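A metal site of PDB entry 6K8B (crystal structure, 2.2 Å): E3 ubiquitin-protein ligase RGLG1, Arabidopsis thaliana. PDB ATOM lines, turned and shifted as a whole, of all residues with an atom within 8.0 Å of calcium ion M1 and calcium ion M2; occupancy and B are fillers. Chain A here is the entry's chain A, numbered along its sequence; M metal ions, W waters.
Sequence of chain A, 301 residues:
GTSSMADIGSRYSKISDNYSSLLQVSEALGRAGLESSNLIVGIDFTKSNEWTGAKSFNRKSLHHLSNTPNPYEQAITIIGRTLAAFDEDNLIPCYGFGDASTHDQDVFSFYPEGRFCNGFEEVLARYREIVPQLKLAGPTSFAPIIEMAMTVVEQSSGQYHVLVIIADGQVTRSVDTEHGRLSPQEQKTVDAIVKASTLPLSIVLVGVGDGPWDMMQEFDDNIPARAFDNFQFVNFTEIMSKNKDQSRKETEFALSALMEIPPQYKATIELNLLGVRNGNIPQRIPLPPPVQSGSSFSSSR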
ATOM      1  N   SER A  13      25.009 -25.201  30.336  1.00  0.00           N
ATOM      2  CA  SER A  13      23.970 -24.180  30.171  1.00  0.00           C
ATOM      3  C   SER A  13      24.466 -22.990  29.325  1.00  0.00           C
ATOM      4  O   SER A  13      25.662 -22.848  29.092  1.00  0.00           O
ATOM      5  CB  SER A  13      23.487 -23.684  31.543  1.00  0.00           C
ATOM      6  OG  SER A  13      22.464 -22.713  31.405  1.00  0.00           O
ATOM      7  N   LYS A  14      23.547 -22.143  28.884  1.00  0.00           N
ATOM      8  CA  LYS A  14      23.905 -21.041  27.983  1.00  0.00           C
ATOM      9  C   LYS A  14      24.600 -19.889  28.728  1.00  0.00           C
ATOM     10  O   LYS A  14      24.163 -19.499  29.809  1.00  0.00           O
ATOM     11  CB  LYS A  14      22.638 -20.532  27.268  1.00  0.00           C
ATOM     12  CG  LYS A  14      22.848 -19.296  26.413  1.00  0.00           C
ATOM     13  CD  LYS A  14      21.722 -18.284  26.669  1.00  0.00           C
ATOM     14  CE  LYS A  14      22.037 -16.921  26.080  1.00  0.00           C
ATOM     15  NZ  LYS A  14      21.028 -15.886  26.466  1.00  0.00           N
ATOM     16  N   ILE A  15      25.677 -19.362  28.155  1.00  0.00           N
ATOM     17  CA  ILE A  15      26.443 -18.294  28.807  1.00  0.00           C
ATOM     18  C   ILE A  15      26.037 -16.912  28.270  1.00  0.00           C
ATOM     19  O   ILE A  15      26.155 -16.623  27.082  1.00  0.00           O
ATOM     20  CB  ILE A  15      27.969 -18.492  28.624  1.00  0.00           C
ATOM     21  CG1 ILE A  15      28.436 -19.743  29.351  1.00  0.00           C
ATOM     22  CG2 ILE A  15      28.739 -17.293  29.148  1.00  0.00           C
ATOM     23  CD1 ILE A  15      29.862 -20.155  29.002  1.00  0.00           C
ATOM     24  N   SER A  16      25.551 -16.043  29.152  1.00  0.00           N
ATOM     25  CA  SER A  16      25.106 -14.720  28.714  1.00  0.00           C
ATOM     26  C   SER A  16      26.260 -13.723  28.729  1.00  0.00           C
ATOM     27  O   SER A  16      27.387 -14.062  29.097  1.00  0.00           O
ATOM     28  CB  SER A  16      23.954 -14.230  29.591  1.00  0.00           C
ATOM     29  OG  SER A  16      22.887 -15.164  29.579  1.00  0.00           O
ATOM     30  N   ASP A  17      25.961 -12.493  28.330  1.00  0.00           N
ATOM     31  CA  ASP A  17      26.928 -11.391  28.370  1.00  0.00           C
ATOM     32  C   ASP A  17      26.996 -10.801  29.784  1.00  0.00           C
ATOM     33  O   ASP A  17      26.244  -9.900  30.120  1.00  0.00           O
ATOM     34  CB  ASP A  17      26.553 -10.315  27.342  1.00  0.00           C
ATOM     35  CG  ASP A  17      26.820 -10.767  25.890  1.00  0.00           C
ATOM     36  OD1 ASP A  17      27.151 -11.939  25.698  1.00  0.00           O
ATOM     37  OD2 ASP A  17      26.702  -9.952  24.954  1.00  0.00           O
ATOM     38  N   ILE A 203      35.661 -21.843  21.593  1.00  0.00           N
ATOM     39  CA  ILE A 203      35.568 -21.440  20.199  1.00  0.00           C
ATOM     40  C   ILE A 203      35.025 -20.015  20.098  1.00  0.00           C
ATOM     41  O   ILE A 203      34.032 -19.669  20.758  1.00  0.00           O
ATOM     42  CB  ILE A 203      34.679 -22.393  19.385  1.00  0.00           C
ATOM     43  CG1 ILE A 203      35.153 -23.837  19.570  1.00  0.00           C
ATOM     44  CG2 ILE A 203      34.687 -21.994  17.914  1.00  0.00           C
ATOM     45  CD1 ILE A 203      34.129 -24.886  19.128  1.00  0.00           C
ATOM     46  N   MET A 216      25.040 -18.578  13.095  1.00  0.00           N
ATOM     47  CA  MET A 216      26.137 -18.349  14.033  1.00  0.00           C
ATOM     48  C   MET A 216      25.600 -18.066  15.440  1.00  0.00           C
ATOM     49  O   MET A 216      26.125 -18.563  16.436  1.00  0.00           O
ATOM     50  CB  MET A 216      27.030 -17.194  13.569  1.00  0.00           C
ATOM     51  CG  MET A 216      27.679 -17.420  12.202  1.00  0.00           C
ATOM     52  SD  MET A 216      28.636 -18.963  12.049  1.00  0.00           S
ATOM     53  CE  MET A 216      27.423 -20.087  11.348  1.00  0.00           C
ATOM     54  N   GLN A 217      24.511 -17.291  15.512  1.00  0.00           N
ATOM     55  CA  GLN A 217      23.882 -17.004  16.792  1.00  0.00           C
ATOM     56  C   GLN A 217      23.285 -18.260  17.428  1.00  0.00           C
ATOM     57  O   GLN A 217      23.258 -18.384  18.649  1.00  0.00           O
ATOM     58  CB  GLN A 217      22.815 -15.920  16.613  1.00  0.00           C
ATOM     59  CG  GLN A 217      23.424 -14.538  16.423  1.00  0.00           C
ATOM     60  CD  GLN A 217      22.481 -13.529  15.760  1.00  0.00           C
ATOM     61  OE1 GLN A 217      21.412 -13.886  15.257  1.00  0.00           O
ATOM     62  NE2 GLN A 217      22.886 -12.258  15.757  1.00  0.00           N
ATOM     63  N   GLU A 218      22.823 -19.188  16.593  1.00  0.00           N
ATOM     64  CA  GLU A 218      22.345 -20.486  17.086  1.00  0.00           C
ATOM     65  C   GLU A 218      23.478 -21.329  17.661  1.00  0.00           C
ATOM     66  O   GLU A 218      23.303 -21.978  18.681  1.00  0.00           O
ATOM     67  CB  GLU A 218      21.641 -21.273  15.975  1.00  0.00           C
ATOM     68  CG  GLU A 218      20.343 -20.646  15.462  1.00  0.00           C
ATOM     69  CD  GLU A 218      19.246 -20.582  16.514  1.00  0.00           C
ATOM     70  OE1 GLU A 218      19.202 -21.470  17.403  1.00  0.00           O
ATOM     71  OE2 GLU A 218      18.444 -19.629  16.470  1.00  0.00           O
ATOM     72  N   PHE A 219      24.624 -21.339  16.973  1.00  0.00           N
ATOM     73  CA  PHE A 219      25.805 -22.010  17.481  1.00  0.00           C
ATOM     74  C   PHE A 219      26.212 -21.405  18.824  1.00  0.00           C
ATOM     75  O   PHE A 219      26.614 -22.119  19.764  1.00  0.00           O
ATOM     76  CB  PHE A 219      26.979 -21.908  16.494  1.00  0.00           C
ATOM     77  CG  PHE A 219      26.790 -22.705  15.237  1.00  0.00           C
ATOM     78  CD1 PHE A 219      25.792 -23.653  15.135  1.00  0.00           C
ATOM     79  CD2 PHE A 219      27.621 -22.479  14.138  1.00  0.00           C
ATOM     80  CE1 PHE A 219      25.631 -24.383  13.950  1.00  0.00           C
ATOM     81  CE2 PHE A 219      27.463 -23.205  12.966  1.00  0.00           C
ATOM     82  CZ  PHE A 219      26.468 -24.157  12.872  1.00  0.00           C
ATOM     83  N   ASP A 220      26.102 -20.082  18.903  1.00  0.00           N
ATOM     84  CA  ASP A 220      26.427 -19.340  20.101  1.00  0.00           C
ATOM     85  C   ASP A 220      25.526 -19.729  21.282  1.00  0.00           C
ATOM     86  O   ASP A 220      26.014 -20.003  22.369  1.00  0.00           O
ATOM     87  CB  ASP A 220      26.331 -17.831  19.816  1.00  0.00           C
ATOM     88  CG  ASP A 220      26.850 -16.968  20.960  1.00  0.00           C
ATOM     89  OD1 ASP A 220      27.379 -17.503  21.959  1.00  0.00           O
ATOM     90  OD2 ASP A 220      26.722 -15.730  20.865  1.00  0.00           O
ATOM     91  N   ASP A 221      24.215 -19.773  21.043  1.00  0.00           N
ATOM     92  CA  ASP A 221      23.224 -19.758  22.129  1.00  0.00           C
ATOM     93  C   ASP A 221      22.411 -21.031  22.329  1.00  0.00           C
ATOM     94  O   ASP A 221      21.809 -21.221  23.386  1.00  0.00           O
ATOM     95  CB  ASP A 221      22.230 -18.614  21.897  1.00  0.00           C
ATOM     96  CG  ASP A 221      22.878 -17.251  21.975  1.00  0.00           C
ATOM     97  OD1 ASP A 221      23.829 -17.093  22.773  1.00  0.00           O
ATOM     98  OD2 ASP A 221      22.449 -16.338  21.244  1.00  0.00           O
ATOM     99  N   ASN A 222      22.359 -21.908  21.333  1.00  0.00           N
ATOM    100  CA  ASN A 222      21.342 -22.936  21.333  1.00  0.00           C
ATOM    101  C   ASN A 222      21.806 -24.274  20.727  1.00  0.00           C
ATOM    102  O   ASN A 222      21.444 -24.620  19.613  1.00  0.00           O
ATOM    103  CB  ASN A 222      20.097 -22.424  20.583  1.00  0.00           C
ATOM    104  CG  ASN A 222      18.946 -23.426  20.576  1.00  0.00           C
ATOM    105  OD1 ASN A 222      18.783 -24.231  21.505  1.00  0.00           O
ATOM    106  ND2 ASN A 222      18.136 -23.389  19.518  1.00  0.00           N
ATOM    107  N   ARG A 226      25.380 -30.201  23.874  1.00  0.00           N
ATOM    108  CA  ARG A 226      26.775 -30.033  24.301  1.00  0.00           C
ATOM    109  C   ARG A 226      26.863 -29.968  25.828  1.00  0.00           C
ATOM    110  O   ARG A 226      25.874 -29.766  26.507  1.00  0.00           O
ATOM    111  CB  ARG A 226      27.401 -28.795  23.665  1.00  0.00           C
ATOM    112  CG  ARG A 226      26.769 -27.478  24.044  1.00  0.00           C
ATOM    113  CD  ARG A 226      27.406 -26.323  23.297  1.00  0.00           C
ATOM    114  NE  ARG A 226      26.563 -25.129  23.353  1.00  0.00           N
ATOM    115  CZ  ARG A 226      26.792 -24.021  22.667  1.00  0.00           C
ATOM    116  NH1 ARG A 226      27.849 -23.926  21.881  1.00  0.00           N
ATOM    117  NH2 ARG A 226      25.948 -22.990  22.772  1.00  0.00           N
ATOM    118  N   PHE A 228      28.843 -27.943  27.782  1.00  0.00           N
ATOM    119  CA  PHE A 228      28.859 -26.564  28.263  1.00  0.00           C
ATOM    120  C   PHE A 228      28.833 -25.642  27.056  1.00  0.00           C
ATOM    121  O   PHE A 228      29.090 -26.080  25.937  1.00  0.00           O
ATOM    122  CB  PHE A 228      30.079 -26.284  29.158  1.00  0.00           C
ATOM    123  CG  PHE A 228      31.414 -26.267  28.429  1.00  0.00           C
ATOM    124  CD1 PHE A 228      32.060 -27.463  28.109  1.00  0.00           C
ATOM    125  CD2 PHE A 228      32.022 -25.061  28.082  1.00  0.00           C
ATOM    126  CE1 PHE A 228      33.295 -27.451  27.451  1.00  0.00           C
ATOM    127  CE2 PHE A 228      33.243 -25.040  27.424  1.00  0.00           C
ATOM    128  CZ  PHE A 228      33.880 -26.239  27.106  1.00  0.00           C
ATOM    129  N   ASP A 229      28.488 -24.383  27.276  1.00  0.00           N
ATOM    130  CA  ASP A 229      28.459 -23.432  26.173  1.00  0.00           C
ATOM    131  C   ASP A 229      29.879 -23.082  25.757  1.00  0.00           C
ATOM    132  O   ASP A 229      30.543 -22.293  26.419  1.00  0.00           O
ATOM    133  CB  ASP A 229      27.673 -22.185  26.577  1.00  0.00           C
ATOM    134  CG  ASP A 229      27.562 -21.170  25.462  1.00  0.00           C
ATOM    135  OD1 ASP A 229      28.145 -21.396  24.374  1.00  0.00           O
ATOM    136  OD2 ASP A 229      26.912 -20.121  25.692  1.00  0.00           O
ATOM    137  N   ASN A 230      30.338 -23.655  24.628  1.00  0.00           N
ATOM    138  CA  ASN A 230      31.751 -23.562  24.238  1.00  0.00           C
ATOM    139  C   ASN A 230      32.012 -22.674  23.020  1.00  0.00           C
ATOM    140  O   ASN A 230      33.098 -22.712  22.433  1.00  0.00           O
ATOM    141  CB  ASN A 230      32.308 -24.972  23.980  1.00  0.00           C
ATOM    142  CG  ASN A 230      31.569 -25.707  22.852  1.00  0.00           C
ATOM    143  OD1 ASN A 230      30.515 -25.254  22.386  1.00  0.00           O
ATOM    144  ND2 ASN A 230      32.125 -26.843  22.410  1.00  0.00           N
ATOM    145  N   PHE A 231      31.024 -21.878  22.659  1.00  0.00           N
ATOM    146  CA  PHE A 231      31.006 -21.182  21.374  1.00  0.00           C
ATOM    147  C   PHE A 231      30.509 -19.756  21.550  1.00  0.00           C
ATOM    148  O   PHE A 231      29.384 -19.556  21.984  1.00  0.00           O
ATOM    149  CB  PHE A 231      30.102 -21.937  20.378  1.00  0.00           C
ATOM    150  CG  PHE A 231      30.255 -21.492  18.936  1.00  0.00           C
ATOM    151  CD1 PHE A 231      29.682 -20.306  18.485  1.00  0.00           C
ATOM    152  CD2 PHE A 231      30.925 -22.289  18.016  1.00  0.00           C
ATOM    153  CE1 PHE A 231      29.796 -19.898  17.165  1.00  0.00           C
ATOM    154  CE2 PHE A 231      31.045 -21.881  16.680  1.00  0.00           C
ATOM    155  CZ  PHE A 231      30.482 -20.701  16.259  1.00  0.00           C
ATOM    156  N   GLN A 232      31.338 -18.784  21.203  1.00  0.00           N
ATOM    157  CA  GLN A 232      30.955 -17.375  21.177  1.00  0.00           C
ATOM    158  C   GLN A 232      30.974 -16.829  19.743  1.00  0.00           C
ATOM    159  O   GLN A 232      31.875 -17.140  18.962  1.00  0.00           O
ATOM    160  CB  GLN A 232      31.884 -16.552  22.074  1.00  0.00           C
ATOM    161  CG  GLN A 232      31.865 -15.048  21.860  1.00  0.00           C
ATOM    162  CD  GLN A 232      30.569 -14.376  22.313  1.00  0.00           C
ATOM    163  OE1 GLN A 232      29.501 -14.979  22.308  1.00  0.00           O
ATOM    164  NE2 GLN A 232      30.669 -13.102  22.720  1.00  0.00           N
ATOM    165  N   PHE A 233      29.960 -16.031  19.408  1.00  0.00           N
ATOM    166  CA  PHE A 233      29.904 -15.353  18.120  1.00  0.00           C
ATOM    167  C   PHE A 233      30.234 -13.863  18.261  1.00  0.00           C
ATOM    168  O   PHE A 233      29.597 -13.159  19.053  1.00  0.00           O
ATOM    169  CB  PHE A 233      28.529 -15.527  17.483  1.00  0.00           C
ATOM    170  CG  PHE A 233      28.280 -14.588  16.331  1.00  0.00           C
ATOM    171  CD1 PHE A 233      29.110 -14.599  15.227  1.00  0.00           C
ATOM    172  CD2 PHE A 233      27.214 -13.692  16.372  1.00  0.00           C
ATOM    173  CE1 PHE A 233      28.889 -13.723  14.164  1.00  0.00           C
ATOM    174  CE2 PHE A 233      26.984 -12.820  15.311  1.00  0.00           C
ATOM    175  CZ  PHE A 233      27.828 -12.840  14.208  1.00  0.00           C
ATOM    176  N   VAL A 234      31.233 -13.395  17.532  1.00  0.00           N
ATOM    177  CA  VAL A 234      31.553 -11.970  17.470  1.00  0.00           C
ATOM    178  C   VAL A 234      31.188 -11.391  16.093  1.00  0.00           C
ATOM    179  O   VAL A 234      31.726 -11.826  15.074  1.00  0.00           O
ATOM    180  CB  VAL A 234      33.033 -11.694  17.715  1.00  0.00           C
ATOM    181  CG1 VAL A 234      33.310 -10.196  17.601  1.00  0.00           C
ATOM    182  CG2 VAL A 234      33.495 -12.260  19.064  1.00  0.00           C
ATOM    183  N   SER A 256      33.976  -8.538  23.364  1.00  0.00           N
ATOM    184  CA  SER A 256      33.096  -9.516  22.705  1.00  0.00           C
ATOM    185  C   SER A 256      33.766 -10.885  22.550  1.00  0.00           C
ATOM    186  O   SER A 256      33.144 -11.910  22.817  1.00  0.00           O
ATOM    187  CB  SER A 256      32.649  -9.012  21.327  1.00  0.00           C
ATOM    188  OG  SER A 256      32.090  -7.717  21.424  1.00  0.00           O
ATOM    189  N   MET A 259      34.234 -12.633  26.016  1.00  0.00           N
ATOM    190  CA  MET A 259      33.043 -12.550  26.877  1.00  0.00           C
ATOM    191  C   MET A 259      32.745 -13.829  27.640  1.00  0.00           C
ATOM    192  O   MET A 259      32.350 -13.789  28.795  1.00  0.00           O
ATOM    193  CB  MET A 259      31.809 -12.162  26.042  1.00  0.00           C
ATOM    194  CG  MET A 259      30.514 -11.932  26.848  1.00  0.00           C
ATOM    195  SD  MET A 259      30.561 -10.468  27.942  1.00  0.00           S
ATOM    196  CE  MET A 259      30.390  -9.118  26.753  1.00  0.00           C
ATOM    197  N   GLU A 260      32.933 -14.978  26.974  1.00  0.00           N
ATOM    198  CA  GLU A 260      32.562 -16.247  27.567  1.00  0.00           C
ATOM    199  C   GLU A 260      33.762 -17.017  28.087  1.00  0.00           C
ATOM    200  O   GLU A 260      33.624 -18.136  28.573  1.00  0.00           O
ATOM    201  CB  GLU A 260      31.803 -17.107  26.554  1.00  0.00           C
ATOM    202  CG  GLU A 260      30.575 -16.437  25.957  1.00  0.00           C
ATOM    203  CD  GLU A 260      29.734 -17.389  25.119  1.00  0.00           C
ATOM    204  OE1 GLU A 260      29.953 -18.613  25.202  1.00  0.00           O
ATOM    205  OE2 GLU A 260      28.846 -16.908  24.377  1.00  0.00           O
ATOM    206  N   GLN A 264      33.859 -20.380  30.484  1.00  0.00           N
ATOM    207  CA  GLN A 264      34.225 -21.575  29.718  1.00  0.00           C
ATOM    208  C   GLN A 264      35.452 -22.225  30.340  1.00  0.00           C
ATOM    209  O   GLN A 264      35.491 -23.439  30.540  1.00  0.00           O
ATOM    210  CB  GLN A 264      34.479 -21.252  28.235  1.00  0.00           C
ATOM    211  CG  GLN A 264      33.188 -21.093  27.478  1.00  0.00           C
ATOM    212  CD  GLN A 264      33.371 -20.514  26.081  1.00  0.00           C
ATOM    213  OE1 GLN A 264      34.465 -20.148  25.672  1.00  0.00           O
ATOM    214  NE2 GLN A 264      32.265 -20.419  25.348  1.00  0.00           N
HETATM  215 CA    CA M   1      27.818 -19.034  23.662  1.00  0.00          CA
HETATM  216 CA    CA M   2      27.463 -15.383  23.354  1.00  0.00          CA
HETATM  217  O   HOH W   1      27.554 -12.946  23.011  1.00  0.00           O
HETATM  218  O   HOH W   2      27.307 -14.522  25.743  1.00  0.00           O
HETATM  219  O   HOH W   3      25.088 -14.871  23.143  1.00  0.00           O
HETATM  220  O   HOH W   4      25.994 -17.387  24.405  1.00  0.00           O
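The side-chain carboxylate (OE2) of Glu 260 is bound to calcium ion M2, at 2.3 Å.
Calcium ion M2 is bound by OE1 of Gln 232, at 2.3 Å.
Water W3 is bound to calcium ion M2.
Calcium ion M2 is bound by water W1 (2.5 Å).
OD1 of Asp 220 binds calcium ion M2.
Water W2 is bound to calcium ion M2, 2.5 Å away.
Calcium ion M2 is bound by OD2 of Asp 220 (2.6 Å).
Water W4 binds calcium ion M2 (2.7 Å).
The nearest printed residue that does not touch calcium ion M1 is Gln 232 (4.3 Å).
Three residues have an atom within 4 Å of calcium ion M2: Asp 220, Gln 232 and Glu 260.
The nearest printed residue that does not touch calcium ion M2 is Asp 221 (4.1 Å).
Water W4 bridges OD1 of Asp 221 (2.7 Å) and O of Ile 15 (2.8 Å).
Water W1 lies within hydrogen-bond range of OD1 of Asp 17 and NE2 of Gln 232.
The side-chain carboxylate of Asp 229 lies close to the guanidinium group of Arg 226 (3.2 Å).
NE2 of Gln 264 lies close to OE1 of Glu 260, 2.9 Å away.
The guanidinium group (NH2) of Arg 226 sits close to the backbone carbonyl oxygen (O) of Asp 220 (3.0 Å).
N of Gln 232 is in hydrogen-bond range of O of Ile 203.
OD2 of Asp 229 lies close to N of Ile 15 (2.9 Å).
O of Ser 256 is in hydrogen-bond range of NE2 of Gln 232 (2.7 Å).
The backbone carbonyl oxygen of Asp 229 sits at hydrogen-bond distance from the side-chain amide nitrogen of Gln 264, at 2.8 Å.
The backbone NH (N) of Phe 231 sits close to the side-chain amide nitrogen (NE2) of Gln 264, at 3.3 Å.
Calcium ion M1 is bound by OD1 of Asp 220 (2.3 Å), O of Phe 231 (2.4 Å), O of Asp 220 (2.4 Å), OE2 of Glu 260 (2.5 Å), OD2 of Asp 229 (2.5 Å), OD1 of Asp 229 (2.5 Å), water W4 (2.6 Å) and OE1 of Glu 260 (2.7 Å).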
